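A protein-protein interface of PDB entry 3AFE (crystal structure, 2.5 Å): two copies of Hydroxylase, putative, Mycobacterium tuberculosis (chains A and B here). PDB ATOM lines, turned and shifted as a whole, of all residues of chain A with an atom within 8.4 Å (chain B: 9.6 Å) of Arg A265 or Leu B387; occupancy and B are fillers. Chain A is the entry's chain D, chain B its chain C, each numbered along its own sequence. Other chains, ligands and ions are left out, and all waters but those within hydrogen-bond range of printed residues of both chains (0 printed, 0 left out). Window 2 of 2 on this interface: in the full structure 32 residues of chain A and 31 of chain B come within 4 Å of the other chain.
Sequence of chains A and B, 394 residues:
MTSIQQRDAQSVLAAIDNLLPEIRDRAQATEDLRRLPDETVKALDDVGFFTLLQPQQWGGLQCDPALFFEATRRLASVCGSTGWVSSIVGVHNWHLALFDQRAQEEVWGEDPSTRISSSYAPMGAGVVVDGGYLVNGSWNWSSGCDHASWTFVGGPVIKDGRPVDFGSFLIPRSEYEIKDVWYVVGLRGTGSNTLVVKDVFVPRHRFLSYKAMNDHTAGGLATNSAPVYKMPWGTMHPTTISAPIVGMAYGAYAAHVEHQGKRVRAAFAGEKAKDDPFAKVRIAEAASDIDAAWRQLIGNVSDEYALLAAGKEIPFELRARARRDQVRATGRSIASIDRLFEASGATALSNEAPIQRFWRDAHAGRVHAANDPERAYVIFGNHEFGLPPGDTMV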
ATOM      1  N   VAL A 257       3.426  27.993   5.184  1.00  0.00           N
ATOM      2  CA  VAL A 257       3.696  27.696   3.784  1.00  0.00           C
ATOM      3  C   VAL A 257       3.717  28.979   2.962  1.00  0.00           C
ATOM      4  O   VAL A 257       4.553  29.137   2.078  1.00  0.00           O
ATOM      5  CB  VAL A 257       2.671  26.693   3.190  1.00  0.00           C
ATOM      6  CG1 VAL A 257       2.713  26.716   1.662  1.00  0.00           C
ATOM      7  CG2 VAL A 257       2.926  25.284   3.719  1.00  0.00           C
ATOM      8  N   GLU A 258       2.806  29.898   3.259  1.00  0.00           N
ATOM      9  CA  GLU A 258       2.772  31.158   2.531  1.00  0.00           C
ATOM     10  C   GLU A 258       4.078  31.903   2.753  1.00  0.00           C
ATOM     11  O   GLU A 258       4.671  32.436   1.809  1.00  0.00           O
ATOM     12  CB  GLU A 258       1.592  32.027   2.966  1.00  0.00           C
ATOM     13  CG  GLU A 258       1.543  33.370   2.255  1.00  0.00           C
ATOM     14  CD  GLU A 258       0.590  34.353   2.920  1.00  0.00           C
ATOM     15  OE1 GLU A 258       0.195  34.102   4.084  1.00  0.00           O
ATOM     16  OE2 GLU A 258       0.238  35.375   2.284  1.00  0.00           O
ATOM     17  N   HIS A 259       4.528  31.921   4.006  1.00  0.00           N
ATOM     18  CA  HIS A 259       5.767  32.607   4.379  1.00  0.00           C
ATOM     19  C   HIS A 259       7.009  31.940   3.788  1.00  0.00           C
ATOM     20  O   HIS A 259       7.845  32.600   3.168  1.00  0.00           O
ATOM     21  CB  HIS A 259       5.880  32.700   5.908  1.00  0.00           C
ATOM     22  CG  HIS A 259       7.289  32.758   6.420  1.00  0.00           C
ATOM     23  ND1 HIS A 259       8.035  33.919   6.425  1.00  0.00           N
ATOM     24  CD2 HIS A 259       8.078  31.803   6.974  1.00  0.00           C
ATOM     25  CE1 HIS A 259       9.226  33.673   6.947  1.00  0.00           C
ATOM     26  NE2 HIS A 259       9.277  32.398   7.288  1.00  0.00           N
ATOM     27  N   GLN A 260       7.117  30.630   3.980  1.00  0.00           N
ATOM     28  CA  GLN A 260       8.300  29.886   3.572  1.00  0.00           C
ATOM     29  C   GLN A 260       8.393  29.795   2.052  1.00  0.00           C
ATOM     30  O   GLN A 260       9.489  29.788   1.487  1.00  0.00           O
ATOM     31  CB  GLN A 260       8.296  28.487   4.203  1.00  0.00           C
ATOM     32  CG  GLN A 260       9.656  27.798   4.209  1.00  0.00           C
ATOM     33  CD  GLN A 260      10.708  28.595   4.962  1.00  0.00           C
ATOM     34  OE1 GLN A 260      10.429  29.182   6.011  1.00  0.00           O
ATOM     35  NE2 GLN A 260      11.927  28.616   4.428  1.00  0.00           N
ATOM     36  N   GLY A 261       7.236  29.738   1.402  1.00  0.00           N
ATOM     37  CA  GLY A 261       7.158  29.643  -0.045  1.00  0.00           C
ATOM     38  C   GLY A 261       7.776  30.820  -0.778  1.00  0.00           C
ATOM     39  O   GLY A 261       8.439  30.640  -1.795  1.00  0.00           O
ATOM     40  N   LYS A 262       7.550  32.028  -0.275  1.00  0.00           N
ATOM     41  CA  LYS A 262       8.170  33.208  -0.859  1.00  0.00           C
ATOM     42  C   LYS A 262       9.683  33.135  -0.710  1.00  0.00           C
ATOM     43  O   LYS A 262      10.419  33.746  -1.479  1.00  0.00           O
ATOM     44  CB  LYS A 262       7.643  34.485  -0.204  1.00  0.00           C
ATOM     45  CG  LYS A 262       6.245  34.875  -0.640  1.00  0.00           C
ATOM     46  CD  LYS A 262       5.683  35.997   0.232  1.00  0.00           C
ATOM     47  CE  LYS A 262       5.523  35.557   1.684  1.00  0.00           C
ATOM     48  NZ  LYS A 262       4.848  36.584   2.531  1.00  0.00           N
ATOM     49  N   ARG A 263      10.146  32.382   0.277  1.00  0.00           N
ATOM     50  CA  ARG A 263      11.576  32.283   0.524  1.00  0.00           C
ATOM     51  C   ARG A 263      12.281  31.257  -0.364  1.00  0.00           C
ATOM     52  O   ARG A 263      13.356  31.535  -0.894  1.00  0.00           O
ATOM     53  CB  ARG A 263      11.835  31.990   1.999  1.00  0.00           C
ATOM     54  CG  ARG A 263      11.382  33.115   2.913  1.00  0.00           C
ATOM     55  CD  ARG A 263      12.543  34.001   3.321  1.00  0.00           C
ATOM     56  NE  ARG A 263      12.966  33.740   4.694  1.00  0.00           N
ATOM     57  CZ  ARG A 263      13.508  32.600   5.112  1.00  0.00           C
ATOM     58  NH1 ARG A 263      13.688  31.593   4.265  1.00  0.00           N
ATOM     59  NH2 ARG A 263      13.864  32.463   6.384  1.00  0.00           N
ATOM     60  N   VAL A 264      11.692  30.073  -0.530  1.00  0.00           N
ATOM     61  CA  VAL A 264      12.341  29.046  -1.342  1.00  0.00           C
ATOM     62  C   VAL A 264      12.347  29.479  -2.805  1.00  0.00           C
ATOM     63  O   VAL A 264      13.344  29.297  -3.510  1.00  0.00           O
ATOM     64  CB  VAL A 264      11.706  27.647  -1.182  1.00  0.00           C
ATOM     65  CG1 VAL A 264      11.491  27.324   0.292  1.00  0.00           C
ATOM     66  CG2 VAL A 264      10.418  27.552  -1.958  1.00  0.00           C
ATOM     67  N   ARG A 265      11.232  30.054  -3.254  1.00  0.00           N
ATOM     68  CA  ARG A 265      11.217  30.807  -4.499  1.00  0.00           C
ATOM     69  C   ARG A 265      12.034  32.068  -4.233  1.00  0.00           C
ATOM     70  O   ARG A 265      11.994  32.600  -3.125  1.00  0.00           O
ATOM     71  CB  ARG A 265       9.785  31.166  -4.893  1.00  0.00           C
ATOM     72  CG  ARG A 265       8.925  29.969  -5.261  1.00  0.00           C
ATOM     73  CD  ARG A 265       7.570  30.402  -5.814  1.00  0.00           C
ATOM     74  NE  ARG A 265       6.539  30.501  -4.780  1.00  0.00           N
ATOM     75  CZ  ARG A 265       6.218  31.621  -4.141  1.00  0.00           C
ATOM     76  NH1 ARG A 265       6.851  32.752  -4.421  1.00  0.00           N
ATOM     77  NH2 ARG A 265       5.267  31.608  -3.217  1.00  0.00           N
ATOM     78  N   ALA A 266      12.775  32.528  -5.239  1.00  0.00           N
ATOM     79  CA  ALA A 266      13.719  33.641  -5.088  1.00  0.00           C
ATOM     80  C   ALA A 266      15.113  33.118  -4.766  1.00  0.00           C
ATOM     81  O   ALA A 266      16.090  33.507  -5.406  1.00  0.00           O
ATOM     82  CB  ALA A 266      13.256  34.642  -4.025  1.00  0.00           C
ATOM     83  N   ALA A 267      15.199  32.238  -3.771  1.00  0.00           N
ATOM     84  CA  ALA A 267      16.436  31.510  -3.499  1.00  0.00           C
ATOM     85  C   ALA A 267      16.630  30.467  -4.594  1.00  0.00           C
ATOM     86  O   ALA A 267      17.640  29.761  -4.640  1.00  0.00           O
ATOM     87  CB  ALA A 267      16.383  30.851  -2.132  1.00  0.00           C
ATOM     88  N   PHE A 268      15.638  30.396  -5.480  1.00  0.00           N
ATOM     89  CA  PHE A 268      15.643  29.492  -6.624  1.00  0.00           C
ATOM     90  C   PHE A 268      16.331  30.144  -7.828  1.00  0.00           C
ATOM     91  O   PHE A 268      16.121  29.729  -8.972  1.00  0.00           O
ATOM     92  CB  PHE A 268      14.203  29.103  -6.980  1.00  0.00           C
ATOM     93  CG  PHE A 268      14.085  27.805  -7.727  1.00  0.00           C
ATOM     94  CD1 PHE A 268      14.621  26.636  -7.205  1.00  0.00           C
ATOM     95  CD2 PHE A 268      13.416  27.747  -8.943  1.00  0.00           C
ATOM     96  CE1 PHE A 268      14.507  25.434  -7.889  1.00  0.00           C
ATOM     97  CE2 PHE A 268      13.297  26.549  -9.631  1.00  0.00           C
ATOM     98  CZ  PHE A 268      13.843  25.390  -9.103  1.00  0.00           C
ATOM     99  N   ALA A 269      17.147  31.166  -7.564  1.00  0.00           N
ATOM    100  CA  ALA A 269      17.919  31.840  -8.608  1.00  0.00           C
ATOM    101  C   ALA A 269      19.387  32.005  -8.195  1.00  0.00           C
ATOM    102  O   ALA A 269      19.804  33.083  -7.763  1.00  0.00           O
ATOM    103  CB  ALA A 269      17.298  33.191  -8.945  1.00  0.00           C
ATOM    104  N   LYS A 274      20.694  27.973  -2.437  1.00  0.00           N
ATOM    105  CA  LYS A 274      20.948  27.050  -1.333  1.00  0.00           C
ATOM    106  C   LYS A 274      20.518  25.629  -1.657  1.00  0.00           C
ATOM    107  O   LYS A 274      21.349  24.742  -1.878  1.00  0.00           O
ATOM    108  CB  LYS A 274      20.188  27.477  -0.075  1.00  0.00           C
ATOM    109  CG  LYS A 274      20.443  28.890   0.398  1.00  0.00           C
ATOM    110  CD  LYS A 274      19.379  29.845  -0.108  1.00  0.00           C
ATOM    111  CE  LYS A 274      19.362  31.111   0.736  1.00  0.00           C
ATOM    112  NZ  LYS A 274      18.452  32.146   0.177  1.00  0.00           N
ATOM    113  N   ASP A 275      19.198  25.447  -1.669  1.00  0.00           N
ATOM    114  CA  ASP A 275      18.528  24.143  -1.682  1.00  0.00           C
ATOM    115  C   ASP A 275      18.374  23.577  -0.265  1.00  0.00           C
ATOM    116  O   ASP A 275      19.331  23.061   0.327  1.00  0.00           O
ATOM    117  CB  ASP A 275      19.217  23.126  -2.589  1.00  0.00           C
ATOM    118  CG  ASP A 275      18.467  21.808  -2.635  1.00  0.00           C
ATOM    119  OD1 ASP A 275      19.098  20.748  -2.411  1.00  0.00           O
ATOM    120  OD2 ASP A 275      17.236  21.838  -2.870  1.00  0.00           O
ATOM    121  N   LYS A 280      11.208  21.136   3.065  1.00  0.00           N
ATOM    122  CA  LYS A 280      10.131  20.411   2.393  1.00  0.00           C
ATOM    123  C   LYS A 280       9.751  19.148   3.166  1.00  0.00           C
ATOM    124  O   LYS A 280       8.580  18.781   3.262  1.00  0.00           O
ATOM    125  CB  LYS A 280      10.537  20.061   0.960  1.00  0.00           C
ATOM    126  CG  LYS A 280      10.847  21.272   0.094  1.00  0.00           C
ATOM    127  CD  LYS A 280      11.704  20.898  -1.107  1.00  0.00           C
ATOM    128  CE  LYS A 280      12.211  22.148  -1.820  1.00  0.00           C
ATOM    129  NZ  LYS A 280      13.173  21.841  -2.926  1.00  0.00           N
ATOM    130  N   PHE B 316      -2.206  16.768 -10.438  1.00  0.00           N
ATOM    131  CA  PHE B 316      -0.891  16.503  -9.882  1.00  0.00           C
ATOM    132  C   PHE B 316      -0.909  16.521  -8.347  1.00  0.00           C
ATOM    133  O   PHE B 316      -0.294  15.663  -7.704  1.00  0.00           O
ATOM    134  CB  PHE B 316       0.134  17.500 -10.427  1.00  0.00           C
ATOM    135  CG  PHE B 316       1.559  17.148 -10.097  1.00  0.00           C
ATOM    136  CD1 PHE B 316       2.190  16.086 -10.730  1.00  0.00           C
ATOM    137  CD2 PHE B 316       2.270  17.883  -9.158  1.00  0.00           C
ATOM    138  CE1 PHE B 316       3.509  15.758 -10.426  1.00  0.00           C
ATOM    139  CE2 PHE B 316       3.585  17.562  -8.850  1.00  0.00           C
ATOM    140  CZ  PHE B 316       4.206  16.501  -9.487  1.00  0.00           C
ATOM    141  N   ALA B 320       0.958  13.800  -5.830  1.00  0.00           N
ATOM    142  CA  ALA B 320       1.975  14.230  -4.887  1.00  0.00           C
ATOM    143  C   ALA B 320       1.570  13.904  -3.445  1.00  0.00           C
ATOM    144  O   ALA B 320       2.408  13.493  -2.642  1.00  0.00           O
ATOM    145  CB  ALA B 320       2.251  15.709  -5.046  1.00  0.00           C
ATOM    146  N   TYR B 377       9.030  13.388  -0.073  1.00  0.00           N
ATOM    147  CA  TYR B 377       8.694  14.656   0.569  1.00  0.00           C
ATOM    148  C   TYR B 377       9.129  15.862  -0.264  1.00  0.00           C
ATOM    149  O   TYR B 377       8.452  16.895  -0.283  1.00  0.00           O
ATOM    150  CB  TYR B 377       9.265  14.742   1.988  1.00  0.00           C
ATOM    151  CG  TYR B 377       8.699  13.712   2.940  1.00  0.00           C
ATOM    152  CD1 TYR B 377       7.426  13.192   2.747  1.00  0.00           C
ATOM    153  CD2 TYR B 377       9.428  13.272   4.042  1.00  0.00           C
ATOM    154  CE1 TYR B 377       6.896  12.253   3.613  1.00  0.00           C
ATOM    155  CE2 TYR B 377       8.907  12.335   4.921  1.00  0.00           C
ATOM    156  CZ  TYR B 377       7.638  11.829   4.696  1.00  0.00           C
ATOM    157  OH  TYR B 377       7.103  10.904   5.545  1.00  0.00           O
ATOM    158  N   VAL B 378      10.260  15.738  -0.951  1.00  0.00           N
ATOM    159  CA  VAL B 378      10.742  16.825  -1.795  1.00  0.00           C
ATOM    160  C   VAL B 378       9.762  17.082  -2.946  1.00  0.00           C
ATOM    161  O   VAL B 378       9.444  18.232  -3.249  1.00  0.00           O
ATOM    162  CB  VAL B 378      12.184  16.568  -2.302  1.00  0.00           C
ATOM    163  CG1 VAL B 378      12.499  17.408  -3.526  1.00  0.00           C
ATOM    164  CG2 VAL B 378      13.195  16.841  -1.186  1.00  0.00           C
ATOM    165  N   ILE B 379       9.250  16.020  -3.558  1.00  0.00           N
ATOM    166  CA  ILE B 379       8.244  16.187  -4.602  1.00  0.00           C
ATOM    167  C   ILE B 379       7.002  16.946  -4.102  1.00  0.00           C
ATOM    168  O   ILE B 379       6.533  17.884  -4.760  1.00  0.00           O
ATOM    169  CB  ILE B 379       7.810  14.840  -5.196  1.00  0.00           C
ATOM    170  CG1 ILE B 379       9.022  14.090  -5.746  1.00  0.00           C
ATOM    171  CG2 ILE B 379       6.764  15.057  -6.287  1.00  0.00           C
ATOM    172  CD1 ILE B 379       8.808  12.600  -5.869  1.00  0.00           C
ATOM    173  N   PHE B 380       6.474  16.537  -2.947  1.00  0.00           N
ATOM    174  CA  PHE B 380       5.311  17.204  -2.365  1.00  0.00           C
ATOM    175  C   PHE B 380       5.667  18.607  -1.890  1.00  0.00           C
ATOM    176  O   PHE B 380       4.873  19.537  -2.022  1.00  0.00           O
ATOM    177  CB  PHE B 380       4.706  16.403  -1.202  1.00  0.00           C
ATOM    178  CG  PHE B 380       3.633  17.159  -0.448  1.00  0.00           C
ATOM    179  CD1 PHE B 380       3.939  17.856   0.712  1.00  0.00           C
ATOM    180  CD2 PHE B 380       2.330  17.201  -0.925  1.00  0.00           C
ATOM    181  CE1 PHE B 380       2.959  18.565   1.389  1.00  0.00           C
ATOM    182  CE2 PHE B 380       1.351  17.903  -0.256  1.00  0.00           C
ATOM    183  CZ  PHE B 380       1.658  18.585   0.899  1.00  0.00           C
ATOM    184  N   GLY B 381       6.861  18.751  -1.327  1.00  0.00           N
ATOM    185  CA  GLY B 381       7.343  20.049  -0.897  1.00  0.00           C
ATOM    186  C   GLY B 381       7.456  21.000  -2.073  1.00  0.00           C
ATOM    187  O   GLY B 381       7.026  22.148  -1.990  1.00  0.00           O
ATOM    188  N   ASN B 382       8.028  20.530  -3.176  1.00  0.00           N
ATOM    189  CA  ASN B 382       8.116  21.364  -4.364  1.00  0.00           C
ATOM    190  C   ASN B 382       6.730  21.853  -4.756  1.00  0.00           C
ATOM    191  O   ASN B 382       6.523  23.055  -4.933  1.00  0.00           O
ATOM    192  CB  ASN B 382       8.796  20.632  -5.526  1.00  0.00           C
ATOM    193  CG  ASN B 382      10.296  20.453  -5.310  1.00  0.00           C
ATOM    194  OD1 ASN B 382      10.944  21.272  -4.655  1.00  0.00           O
ATOM    195  ND2 ASN B 382      10.852  19.375  -5.865  1.00  0.00           N
ATOM    196  N   HIS B 383       5.774  20.933  -4.855  1.00  0.00           N
ATOM    197  CA  HIS B 383       4.425  21.306  -5.283  1.00  0.00           C
ATOM    198  C   HIS B 383       3.735  22.354  -4.390  1.00  0.00           C
ATOM    199  O   HIS B 383       3.064  23.251  -4.894  1.00  0.00           O
ATOM    200  CB  HIS B 383       3.527  20.080  -5.443  1.00  0.00           C
ATOM    201  CG  HIS B 383       2.104  20.419  -5.762  1.00  0.00           C
ATOM    202  ND1 HIS B 383       1.228  20.907  -4.816  1.00  0.00           N
ATOM    203  CD2 HIS B 383       1.405  20.346  -6.920  1.00  0.00           C
ATOM    204  CE1 HIS B 383       0.049  21.118  -5.377  1.00  0.00           C
ATOM    205  NE2 HIS B 383       0.128  20.782  -6.652  1.00  0.00           N
ATOM    206  N   GLU B 384       3.890  22.242  -3.073  1.00  0.00           N
ATOM    207  CA  GLU B 384       3.321  23.239  -2.164  1.00  0.00           C
ATOM    208  C   GLU B 384       4.005  24.602  -2.302  1.00  0.00           C
ATOM    209  O   GLU B 384       3.377  25.642  -2.090  1.00  0.00           O
ATOM    210  CB  GLU B 384       3.413  22.783  -0.703  1.00  0.00           C
ATOM    211  CG  GLU B 384       2.597  21.559  -0.351  1.00  0.00           C
ATOM    212  CD  GLU B 384       1.107  21.834  -0.307  1.00  0.00           C
ATOM    213  OE1 GLU B 384       0.569  22.064   0.806  1.00  0.00           O
ATOM    214  OE2 GLU B 384       0.479  21.816  -1.388  1.00  0.00           O
ATOM    215  N   PHE B 385       5.293  24.595  -2.643  1.00  0.00           N
ATOM    216  CA  PHE B 385       6.065  25.832  -2.704  1.00  0.00           C
ATOM    217  C   PHE B 385       5.998  26.537  -4.062  1.00  0.00           C
ATOM    218  O   PHE B 385       6.661  27.553  -4.264  1.00  0.00           O
ATOM    219  CB  PHE B 385       7.524  25.582  -2.324  1.00  0.00           C
ATOM    220  CG  PHE B 385       7.760  25.514  -0.848  1.00  0.00           C
ATOM    221  CD1 PHE B 385       8.734  24.676  -0.326  1.00  0.00           C
ATOM    222  CD2 PHE B 385       7.006  26.279   0.022  1.00  0.00           C
ATOM    223  CE1 PHE B 385       8.955  24.609   1.024  1.00  0.00           C
ATOM    224  CE2 PHE B 385       7.228  26.215   1.376  1.00  0.00           C
ATOM    225  CZ  PHE B 385       8.200  25.383   1.875  1.00  0.00           C
ATOM    226  N   GLY B 386       5.203  25.999  -4.983  1.00  0.00           N
ATOM    227  CA  GLY B 386       5.038  26.604  -6.296  1.00  0.00           C
ATOM    228  C   GLY B 386       6.197  26.333  -7.246  1.00  0.00           C
ATOM    229  O   GLY B 386       6.491  27.147  -8.124  1.00  0.00           O
ATOM    230  N   LEU B 387       6.848  25.185  -7.069  1.00  0.00           N
ATOM    231  CA  LEU B 387       8.007  24.810  -7.871  1.00  0.00           C
ATOM    232  C   LEU B 387       7.654  23.781  -8.937  1.00  0.00           C
ATOM    233  O   LEU B 387       6.714  22.994  -8.764  1.00  0.00           O
ATOM    234  CB  LEU B 387       9.118  24.254  -6.977  1.00  0.00           C
ATOM    235  CG  LEU B 387      10.204  25.207  -6.480  1.00  0.00           C
ATOM    236  CD1 LEU B 387       9.701  26.643  -6.371  1.00  0.00           C
ATOM    237  CD2 LEU B 387      10.733  24.728  -5.141  1.00  0.00           C
ATOM    238  N   PRO B 388       8.415  23.788 -10.045  1.00  0.00           N
ATOM    239  CA  PRO B 388       8.270  22.820 -11.135  1.00  0.00           C
ATOM    240  C   PRO B 388       8.587  21.418 -10.655  1.00  0.00           C
ATOM    241  O   PRO B 388       9.489  21.230  -9.834  1.00  0.00           O
ATOM    242  CB  PRO B 388       9.337  23.272 -12.143  1.00  0.00           C
ATOM    243  CG  PRO B 388      10.320  24.063 -11.312  1.00  0.00           C
ATOM    244  CD  PRO B 388       9.429  24.806 -10.370  1.00  0.00           C
ATOM    245  N   PRO B 389       7.838  20.433 -11.159  1.00  0.00           N
ATOM    246  CA  PRO B 389       8.081  19.024 -10.837  1.00  0.00           C
ATOM    247  C   PRO B 389       9.435  18.548 -11.372  1.00  0.00           C
ATOM    248  O   PRO B 389       9.925  19.073 -12.375  1.00  0.00           O
ATOM    249  CB  PRO B 389       6.939  18.300 -11.563  1.00  0.00           C
ATOM    250  CG  PRO B 389       5.890  19.363 -11.811  1.00  0.00           C
ATOM    251  CD  PRO B 389       6.659  20.622 -12.023  1.00  0.00           C
ATOM    252  N   GLY B 390      10.030  17.568 -10.698  1.00  0.00           N
ATOM    253  CA  GLY B 390      11.241  16.924 -11.180  1.00  0.00           C
ATOM    254  C   GLY B 390      11.087  15.408 -11.195  1.00  0.00           C
ATOM    255  O   GLY B 390      10.505  14.843 -12.128  1.00  0.00           O
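The side-chain amino group (NZ) of Lys A280 sits at hydrogen-bond distance from the side-chain amide oxygen (OD1) of Asn B382 (2.9 Å).
The guanidinium group (NE) of Arg A265 sits at hydrogen-bond distance from the backbone carbonyl oxygen (O) of Phe B385, at 3.0 Å.
O of Val B378 sits close to ND2 of Asn B382, at 3.2 Å.
The backbone NH of Leu B387 sits at hydrogen-bond distance from the backbone carbonyl oxygen of Asn B382, at 3.0 Å.
The side-chain amide nitrogen of Gln A260 lies close to the guanidinium group of Arg A263, at 3.5 Å.
Glu B384 touches Val A257.
Gln A260 touches Phe B385.
CA of Gly A261 touches CD2 of Phe B385 (3.4 Å).
Val A264 touches Phe B385 (CG2 to CB, 3.5 Å).
Leu B387 touches Arg A265.
O of Tyr B377 touches CB of Lys A280 (3.99 Å).
Lys A280 touches Gly B381 (CB to CA, 3.7 Å).
Phe B385 touches Lys A280 (CE1 to CG, 3.9 Å).
Arg A265 touches two residues of chain B.
Leu B387 touches one residue of chain A.
Of chain B, only Phe B385 comes within 4 Å of Gly A261.
Val A264 touches just one residue of chain B: Phe B385 (3.5 Å).
Ala A266 touches none of the printed residues of chain B.
No residue of chain A comes within 4 Å of Gly B386.
No residue of chain A comes within 4 Å of Pro B388.
Printed residues of chain B within 4 Å of Lys A280: Tyr B377, Gly B381, Asn B382 and Phe B385.
Of the printed residues of chain B, Val A257 touches Glu B384 (3.96 Å).
Printed residues of chain A within 4 Å of Gly B381: Lys A280.
Printed residues of chain A within 4 Å of Glu B384: Val A257 (3.96 Å).
Of the printed residues of chain A, Tyr B377 touches Lys A280 (3.99 Å).
Asp A275 touches none of the printed residues of chain B.
Lys A274 touches none of the printed residues of chain B.
The nearest residue of chain B that does not touch Arg A265 is Gly B386 (4.1 Å).
The nearest residue of chain A that does not touch Leu B387 is Val A264 (4.3 Å).
The nearest printed residue of chain A that does not touch Asn B382 is Phe A268 (6.4 Å).
Hydrophobic or aromatic side chains of chain B that line the printed part of chain A: Phe B385 and Leu B387.
Along chain B the printed residues that touch a printed residue of chain A span positions 377 to 387.
Among the printed residues, 10 pairs touch across the chains.
No position is printed for both chains.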
